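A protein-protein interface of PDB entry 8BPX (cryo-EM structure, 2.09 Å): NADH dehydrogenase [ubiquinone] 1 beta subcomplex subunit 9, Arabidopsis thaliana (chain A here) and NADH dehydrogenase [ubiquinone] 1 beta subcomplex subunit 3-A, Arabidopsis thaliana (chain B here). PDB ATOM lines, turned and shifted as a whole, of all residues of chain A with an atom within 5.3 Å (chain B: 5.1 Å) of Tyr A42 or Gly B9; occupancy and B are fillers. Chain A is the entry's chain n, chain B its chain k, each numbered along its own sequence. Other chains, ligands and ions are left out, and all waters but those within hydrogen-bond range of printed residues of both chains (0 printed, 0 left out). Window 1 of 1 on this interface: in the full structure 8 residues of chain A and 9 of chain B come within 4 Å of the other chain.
N of Gly B6 is in hydrogen-bond range of OG of Ser A46 (3.3 Å).
The backbone NH (N) of Gly B9 is in hydrogen-bond range of the side-chain hydroxyl (OG) of Ser A46, 3.3 Å away.
The side-chain carboxylate (OD2) of Asp B16 is in salt-bridge range of the guanidinium group (NE) of Arg A38, at 2.9 Å.
The side-chain carboxylate (OD2) of Asp B16 lies within hydrogen-bond range of the side-chain hydroxyl (OH) of Tyr A42.
O of Pro B4 sits at hydrogen-bond distance from N of Glu B10 (3.4 Å).
OE1 of Glu B10 lies within salt-bridge range of NH2 of Arg B13.
The backbone carbonyl oxygen (O) of Tyr A42 sits at hydrogen-bond distance from the side-chain hydroxyl (OG) of Ser A46 (3.3 Å).
CE2 of Phe A41 touches CD2 of Phe B12, at 3.6 Å.
CB of Tyr A42 touches CA of Pro B4, at 3.8 Å.
Tyr A42 touches Gly B9.
CE1 of Tyr A42 touches C of Phe B12, 3.7 Å away.
CA of Arg B13 touches CZ of Tyr A42, at 3.6 Å.
CG2 of Thr B8 touches CB of Ala A45, at 3.9 Å.
Printed residues of chain B within 4 Å of Tyr A42: Pro B4, Gly B9, Phe B12, Arg B13 and Asp B16.
Gly B9 touches two residues of chain A.
Printed residues of chain B within 4 Å of Ala A45: Thr B8 (3.9 Å).
Of the printed residues of chain B, Ser A46 touches Gly B6 and Gly B9.
The nearest printed residue of chain B that does not touch Tyr A42 is Thr B8 (5.2 Å).
Of the 11 printed residues of chain B, 7 touch a printed residue of chain A.
Printed residues of chain A that touch a printed residue of chain B: Arg A38, Phe A41, Tyr A42, Ala A45 and Ser A46.
Among the printed residues, Asp or Glu carboxylates within 4 Å of a Lys or Arg side-chain nitrogen of the other chain: Arg A38 with Asp B16 (2.9 Å).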
ATOM      1  N   ARG A  38      15.233  -1.043   6.105  1.00  0.00           N
ATOM      2  CA  ARG A  38      14.617  -0.570   4.828  1.00  0.00           C
ATOM      3  C   ARG A  38      13.880  -1.671   4.053  1.00  0.00           C
ATOM      4  O   ARG A  38      12.702  -1.504   3.823  1.00  0.00           O
ATOM      5  CB  ARG A  38      15.700   0.106   3.981  1.00  0.00           C
ATOM      6  CG  ARG A  38      16.473   1.223   4.668  1.00  0.00           C
ATOM      7  CD  ARG A  38      15.671   2.352   5.289  1.00  0.00           C
ATOM      8  NE  ARG A  38      14.977   3.138   4.293  1.00  0.00           N
ATOM      9  CZ  ARG A  38      14.226   4.207   4.531  1.00  0.00           C
ATOM     10  NH1 ARG A  38      14.047   4.647   5.761  1.00  0.00           N
ATOM     11  NH2 ARG A  38      13.656   4.834   3.520  1.00  0.00           N
ATOM     12  N   HIS A  39      14.467  -2.848   3.848  1.00  0.00           N
ATOM     13  CA  HIS A  39      13.879  -3.860   2.973  1.00  0.00           C
ATOM     14  C   HIS A  39      12.603  -4.454   3.559  1.00  0.00           C
ATOM     15  O   HIS A  39      11.687  -4.803   2.806  1.00  0.00           O
ATOM     16  CB  HIS A  39      14.901  -4.956   2.659  1.00  0.00           C
ATOM     17  CG  HIS A  39      15.264  -5.807   3.835  1.00  0.00           C
ATOM     18  ND1 HIS A  39      14.563  -6.943   4.174  1.00  0.00           N
ATOM     19  CD2 HIS A  39      16.253  -5.687   4.749  1.00  0.00           C
ATOM     20  CE1 HIS A  39      15.107  -7.486   5.247  1.00  0.00           C
ATOM     21  NE2 HIS A  39      16.131  -6.741   5.619  1.00  0.00           N
ATOM     22  N   ILE A  40      12.548  -4.543   4.893  1.00  0.00           N
ATOM     23  CA  ILE A  40      11.289  -4.992   5.547  1.00  0.00           C
ATOM     24  C   ILE A  40      10.220  -3.882   5.401  1.00  0.00           C
ATOM     25  O   ILE A  40       9.061  -4.222   5.214  1.00  0.00           O
ATOM     26  CB  ILE A  40      11.534  -5.403   7.013  1.00  0.00           C
ATOM     27  CG1 ILE A  40      12.569  -6.526   7.140  1.00  0.00           C
ATOM     28  CG2 ILE A  40      10.248  -5.732   7.751  1.00  0.00           C
ATOM     29  CD1 ILE A  40      13.080  -6.718   8.538  1.00  0.00           C
ATOM     30  N   PHE A  41      10.630  -2.608   5.487  1.00  0.00           N
ATOM     31  CA  PHE A  41       9.706  -1.441   5.336  1.00  0.00           C
ATOM     32  C   PHE A  41       9.045  -1.494   3.951  1.00  0.00           C
ATOM     33  O   PHE A  41       7.862  -1.301   3.878  1.00  0.00           O
ATOM     34  CB  PHE A  41      10.346  -0.081   5.654  1.00  0.00           C
ATOM     35  CG  PHE A  41       9.537   1.150   5.338  1.00  0.00           C
ATOM     36  CD1 PHE A  41       8.398   1.458   6.061  1.00  0.00           C
ATOM     37  CD2 PHE A  41       9.939   2.024   4.341  1.00  0.00           C
ATOM     38  CE1 PHE A  41       7.659   2.594   5.768  1.00  0.00           C
ATOM     39  CE2 PHE A  41       9.205   3.161   4.055  1.00  0.00           C
ATOM     40  CZ  PHE A  41       8.071   3.448   4.774  1.00  0.00           C
ATOM     41  N   TYR A  42       9.811  -1.831   2.930  1.00  0.00           N
ATOM     42  CA  TYR A  42       9.229  -1.829   1.586  1.00  0.00           C
ATOM     43  C   TYR A  42       7.967  -2.686   1.530  1.00  0.00           C
ATOM     44  O   TYR A  42       6.894  -2.221   1.114  1.00  0.00           O
ATOM     45  CB  TYR A  42      10.249  -2.326   0.557  1.00  0.00           C
ATOM     46  CG  TYR A  42      11.574  -1.599   0.549  1.00  0.00           C
ATOM     47  CD1 TYR A  42      11.665  -0.266   0.924  1.00  0.00           C
ATOM     48  CD2 TYR A  42      12.738  -2.247   0.142  1.00  0.00           C
ATOM     49  CE1 TYR A  42      12.874   0.397   0.915  1.00  0.00           C
ATOM     50  CE2 TYR A  42      13.947  -1.594   0.127  1.00  0.00           C
ATOM     51  CZ  TYR A  42      14.011  -0.272   0.512  1.00  0.00           C
ATOM     52  OH  TYR A  42      15.215   0.382   0.496  1.00  0.00           O
ATOM     53  N   ARG A  43       8.090  -3.961   1.910  1.00  0.00           N
ATOM     54  CA  ARG A  43       6.920  -4.847   1.965  1.00  0.00           C
ATOM     55  C   ARG A  43       5.821  -4.349   2.934  1.00  0.00           C
ATOM     56  O   ARG A  43       4.663  -4.403   2.583  1.00  0.00           O
ATOM     57  CB  ARG A  43       7.434  -6.235   2.347  1.00  0.00           C
ATOM     58  CG  ARG A  43       6.380  -7.331   2.305  1.00  0.00           C
ATOM     59  CD  ARG A  43       5.504  -7.337   1.066  1.00  0.00           C
ATOM     60  NE  ARG A  43       6.225  -7.248  -0.194  1.00  0.00           N
ATOM     61  CZ  ARG A  43       6.679  -8.286  -0.886  1.00  0.00           C
ATOM     62  NH1 ARG A  43       6.493  -9.515  -0.441  1.00  0.00           N
ATOM     63  NH2 ARG A  43       7.321  -8.089  -2.024  1.00  0.00           N
ATOM     64  N   ASP A  44       6.196  -3.900   4.100  1.00  0.00           N
ATOM     65  CA  ASP A  44       5.176  -3.472   5.055  1.00  0.00           C
ATOM     66  C   ASP A  44       4.394  -2.270   4.532  1.00  0.00           C
ATOM     67  O   ASP A  44       3.162  -2.212   4.659  1.00  0.00           O
ATOM     68  CB  ASP A  44       5.831  -3.172   6.397  1.00  0.00           C
ATOM     69  CG  ASP A  44       5.941  -4.401   7.274  1.00  0.00           C
ATOM     70  OD1 ASP A  44       5.007  -4.656   8.060  1.00  0.00           O
ATOM     71  OD2 ASP A  44       6.956  -5.120   7.171  1.00  0.00           O
ATOM     72  N   ALA A  45       5.093  -1.312   3.921  1.00  0.00           N
ATOM     73  CA  ALA A  45       4.443  -0.155   3.324  1.00  0.00           C
ATOM     74  C   ALA A  45       3.536  -0.561   2.172  1.00  0.00           C
ATOM     75  O   ALA A  45       2.427  -0.031   2.035  1.00  0.00           O
ATOM     76  CB  ALA A  45       5.499   0.846   2.855  1.00  0.00           C
ATOM     77  N   SER A  46       4.024  -1.453   1.303  1.00  0.00           N
ATOM     78  CA  SER A  46       3.165  -2.001   0.207  1.00  0.00           C
ATOM     79  C   SER A  46       1.878  -2.618   0.761  1.00  0.00           C
ATOM     80  O   SER A  46       0.832  -2.262   0.247  1.00  0.00           O
ATOM     81  CB  SER A  46       3.864  -2.972  -0.627  1.00  0.00           C
ATOM     82  OG  SER A  46       4.805  -2.347  -1.479  1.00  0.00           O
ATOM     83  N   ASP A  47       1.956  -3.405   1.836  1.00  0.00           N
ATOM     84  CA  ASP A  47       0.771  -4.040   2.410  1.00  0.00           C
ATOM     85  C   ASP A  47      -0.189  -3.012   3.006  1.00  0.00           C
ATOM     86  O   ASP A  47      -1.414  -3.123   2.848  1.00  0.00           O
ATOM     87  CB  ASP A  47       1.191  -5.061   3.464  1.00  0.00           C
ATOM     88  CG  ASP A  47       1.841  -6.292   2.860  1.00  0.00           C
ATOM     89  OD1 ASP A  47       1.719  -6.493   1.633  1.00  0.00           O
ATOM     90  OD2 ASP A  47       2.476  -7.060   3.613  1.00  0.00           O
ATOM     91  N   PRO B   4       9.540  -4.761  -2.464  1.00  0.00           N
ATOM     92  CA  PRO B   4       9.398  -3.453  -3.003  1.00  0.00           C
ATOM     93  C   PRO B   4       8.503  -3.777  -4.180  1.00  0.00           C
ATOM     94  O   PRO B   4       8.591  -3.133  -5.176  1.00  0.00           O
ATOM     95  CB  PRO B   4      10.775  -2.902  -3.366  1.00  0.00           C
ATOM     96  CG  PRO B   4      11.682  -4.099  -3.159  1.00  0.00           C
ATOM     97  CD  PRO B   4      10.959  -4.990  -2.173  1.00  0.00           C
ATOM     98  N   GLY B   6       5.055  -3.637  -4.455  1.00  0.00           N
ATOM     99  CA  GLY B   6       4.059  -2.566  -4.656  1.00  0.00           C
ATOM    100  C   GLY B   6       4.645  -1.233  -5.050  1.00  0.00           C
ATOM    101  O   GLY B   6       5.814  -1.014  -4.797  1.00  0.00           O
ATOM    102  N   THR B   7       3.825  -0.385  -5.652  1.00  0.00           N
ATOM    103  CA  THR B   7       4.315   0.925  -6.070  1.00  0.00           C
ATOM    104  C   THR B   7       4.967   1.680  -4.911  1.00  0.00           C
ATOM    105  O   THR B   7       5.995   2.340  -5.095  1.00  0.00           O
ATOM    106  CB  THR B   7       3.176   1.733  -6.710  1.00  0.00           C
ATOM    107  OG1 THR B   7       3.718   2.828  -7.455  1.00  0.00           O
ATOM    108  CG2 THR B   7       2.184   2.259  -5.675  1.00  0.00           C
ATOM    109  N   THR B   8       4.418   1.550  -3.702  1.00  0.00           N
ATOM    110  CA  THR B   8       4.961   2.266  -2.550  1.00  0.00           C
ATOM    111  C   THR B   8       6.351   1.754  -2.180  1.00  0.00           C
ATOM    112  O   THR B   8       7.302   2.537  -2.035  1.00  0.00           O
ATOM    113  CB  THR B   8       3.999   2.127  -1.370  1.00  0.00           C
ATOM    114  OG1 THR B   8       2.682   2.494  -1.788  1.00  0.00           O
ATOM    115  CG2 THR B   8       4.425   3.012  -0.213  1.00  0.00           C
ATOM    116  N   GLY B   9       6.485   0.435  -2.030  1.00  0.00           N
ATOM    117  CA  GLY B   9       7.783  -0.135  -1.714  1.00  0.00           C
ATOM    118  C   GLY B   9       8.795   0.077  -2.820  1.00  0.00           C
ATOM    119  O   GLY B   9       9.982   0.264  -2.558  1.00  0.00           O
ATOM    120  N   GLU B  10       8.336   0.049  -4.071  1.00  0.00           N
ATOM    121  CA  GLU B  10       9.217   0.301  -5.204  1.00  0.00           C
ATOM    122  C   GLU B  10       9.749   1.728  -5.183  1.00  0.00           C
ATOM    123  O   GLU B  10      10.938   1.960  -5.426  1.00  0.00           O
ATOM    124  CB  GLU B  10       8.465   0.015  -6.503  1.00  0.00           C
ATOM    125  CG  GLU B  10       9.013   0.718  -7.730  1.00  0.00           C
ATOM    126  CD  GLU B  10      10.415   0.287  -8.085  1.00  0.00           C
ATOM    127  OE1 GLU B  10      10.821  -0.829  -7.694  1.00  0.00           O
ATOM    128  OE2 GLU B  10      11.112   1.067  -8.763  1.00  0.00           O
ATOM    129  N   PHE B  11       8.882   2.696  -4.885  1.00  0.00           N
ATOM    130  CA  PHE B  11       9.319   4.080  -4.767  1.00  0.00           C
ATOM    131  C   PHE B  11      10.331   4.241  -3.639  1.00  0.00           C
ATOM    132  O   PHE B  11      11.372   4.896  -3.805  1.00  0.00           O
ATOM    133  CB  PHE B  11       8.093   4.967  -4.551  1.00  0.00           C
ATOM    134  CG  PHE B  11       8.409   6.387  -4.210  1.00  0.00           C
ATOM    135  CD1 PHE B  11       9.230   7.145  -5.021  1.00  0.00           C
ATOM    136  CD2 PHE B  11       7.860   6.973  -3.084  1.00  0.00           C
ATOM    137  CE1 PHE B  11       9.510   8.456  -4.706  1.00  0.00           C
ATOM    138  CE2 PHE B  11       8.136   8.290  -2.766  1.00  0.00           C
ATOM    139  CZ  PHE B  11       8.962   9.028  -3.582  1.00  0.00           C
ATOM    140  N   PHE B  12      10.058   3.627  -2.487  1.00  0.00           N
ATOM    141  CA  PHE B  12      10.973   3.791  -1.362  1.00  0.00           C
ATOM    142  C   PHE B  12      12.301   3.074  -1.600  1.00  0.00           C
ATOM    143  O   PHE B  12      13.345   3.558  -1.159  1.00  0.00           O
ATOM    144  CB  PHE B  12      10.304   3.322  -0.076  1.00  0.00           C
ATOM    145  CG  PHE B  12       9.342   4.324   0.487  1.00  0.00           C
ATOM    146  CD1 PHE B  12       9.756   5.617   0.762  1.00  0.00           C
ATOM    147  CD2 PHE B  12       8.020   3.984   0.719  1.00  0.00           C
ATOM    148  CE1 PHE B  12       8.872   6.550   1.270  1.00  0.00           C
ATOM    149  CE2 PHE B  12       7.132   4.916   1.227  1.00  0.00           C
ATOM    150  CZ  PHE B  12       7.557   6.198   1.503  1.00  0.00           C
ATOM    151  N   ARG B  13      12.288   1.941  -2.302  1.00  0.00           N
ATOM    152  CA  ARG B  13      13.539   1.284  -2.666  1.00  0.00           C
ATOM    153  C   ARG B  13      14.321   2.107  -3.683  1.00  0.00           C
ATOM    154  O   ARG B  13      15.552   2.179  -3.614  1.00  0.00           O
ATOM    155  CB  ARG B  13      13.264  -0.112  -3.216  1.00  0.00           C
ATOM    156  CG  ARG B  13      14.525  -0.902  -3.479  1.00  0.00           C
ATOM    157  CD  ARG B  13      14.220  -2.232  -4.139  1.00  0.00           C
ATOM    158  NE  ARG B  13      13.828  -2.166  -5.548  1.00  0.00           N
ATOM    159  CZ  ARG B  13      14.358  -1.391  -6.492  1.00  0.00           C
ATOM    160  NH1 ARG B  13      15.411  -0.621  -6.263  1.00  0.00           N
ATOM    161  NH2 ARG B  13      13.840  -1.420  -7.716  1.00  0.00           N
ATOM    162  N   ARG B  14      13.623   2.735  -4.631  1.00  0.00           N
ATOM    163  CA  ARG B  14      14.295   3.608  -5.585  1.00  0.00           C
ATOM    164  C   ARG B  14      14.983   4.767  -4.881  1.00  0.00           C
ATOM    165  O   ARG B  14      16.106   5.139  -5.238  1.00  0.00           O
ATOM    166  CB  ARG B  14      13.295   4.128  -6.614  1.00  0.00           C
ATOM    167  CG  ARG B  14      13.163   3.252  -7.831  1.00  0.00           C
ATOM    168  CD  ARG B  14      12.588   4.009  -9.001  1.00  0.00           C
ATOM    169  NE  ARG B  14      11.700   3.179  -9.805  1.00  0.00           N
ATOM    170  CZ  ARG B  14      10.689   3.640 -10.525  1.00  0.00           C
ATOM    171  NH1 ARG B  14      10.406   4.931 -10.568  1.00  0.00           N
ATOM    172  NH2 ARG B  14       9.950   2.787 -11.224  1.00  0.00           N
ATOM    173  N   ASP B  16      16.241   4.737  -1.983  1.00  0.00           N
ATOM    174  CA  ASP B  16      17.310   4.228  -1.136  1.00  0.00           C
ATOM    175  C   ASP B  16      18.529   3.757  -1.924  1.00  0.00           C
ATOM    176  O   ASP B  16      19.362   3.037  -1.369  1.00  0.00           O
ATOM    177  CB  ASP B  16      16.796   3.072  -0.270  1.00  0.00           C
ATOM    178  CG  ASP B  16      16.059   3.543   0.971  1.00  0.00           C
ATOM    179  OD1 ASP B  16      16.471   4.556   1.566  1.00  0.00           O
ATOM    180  OD2 ASP B  16      15.079   2.886   1.364  1.00  0.00           O
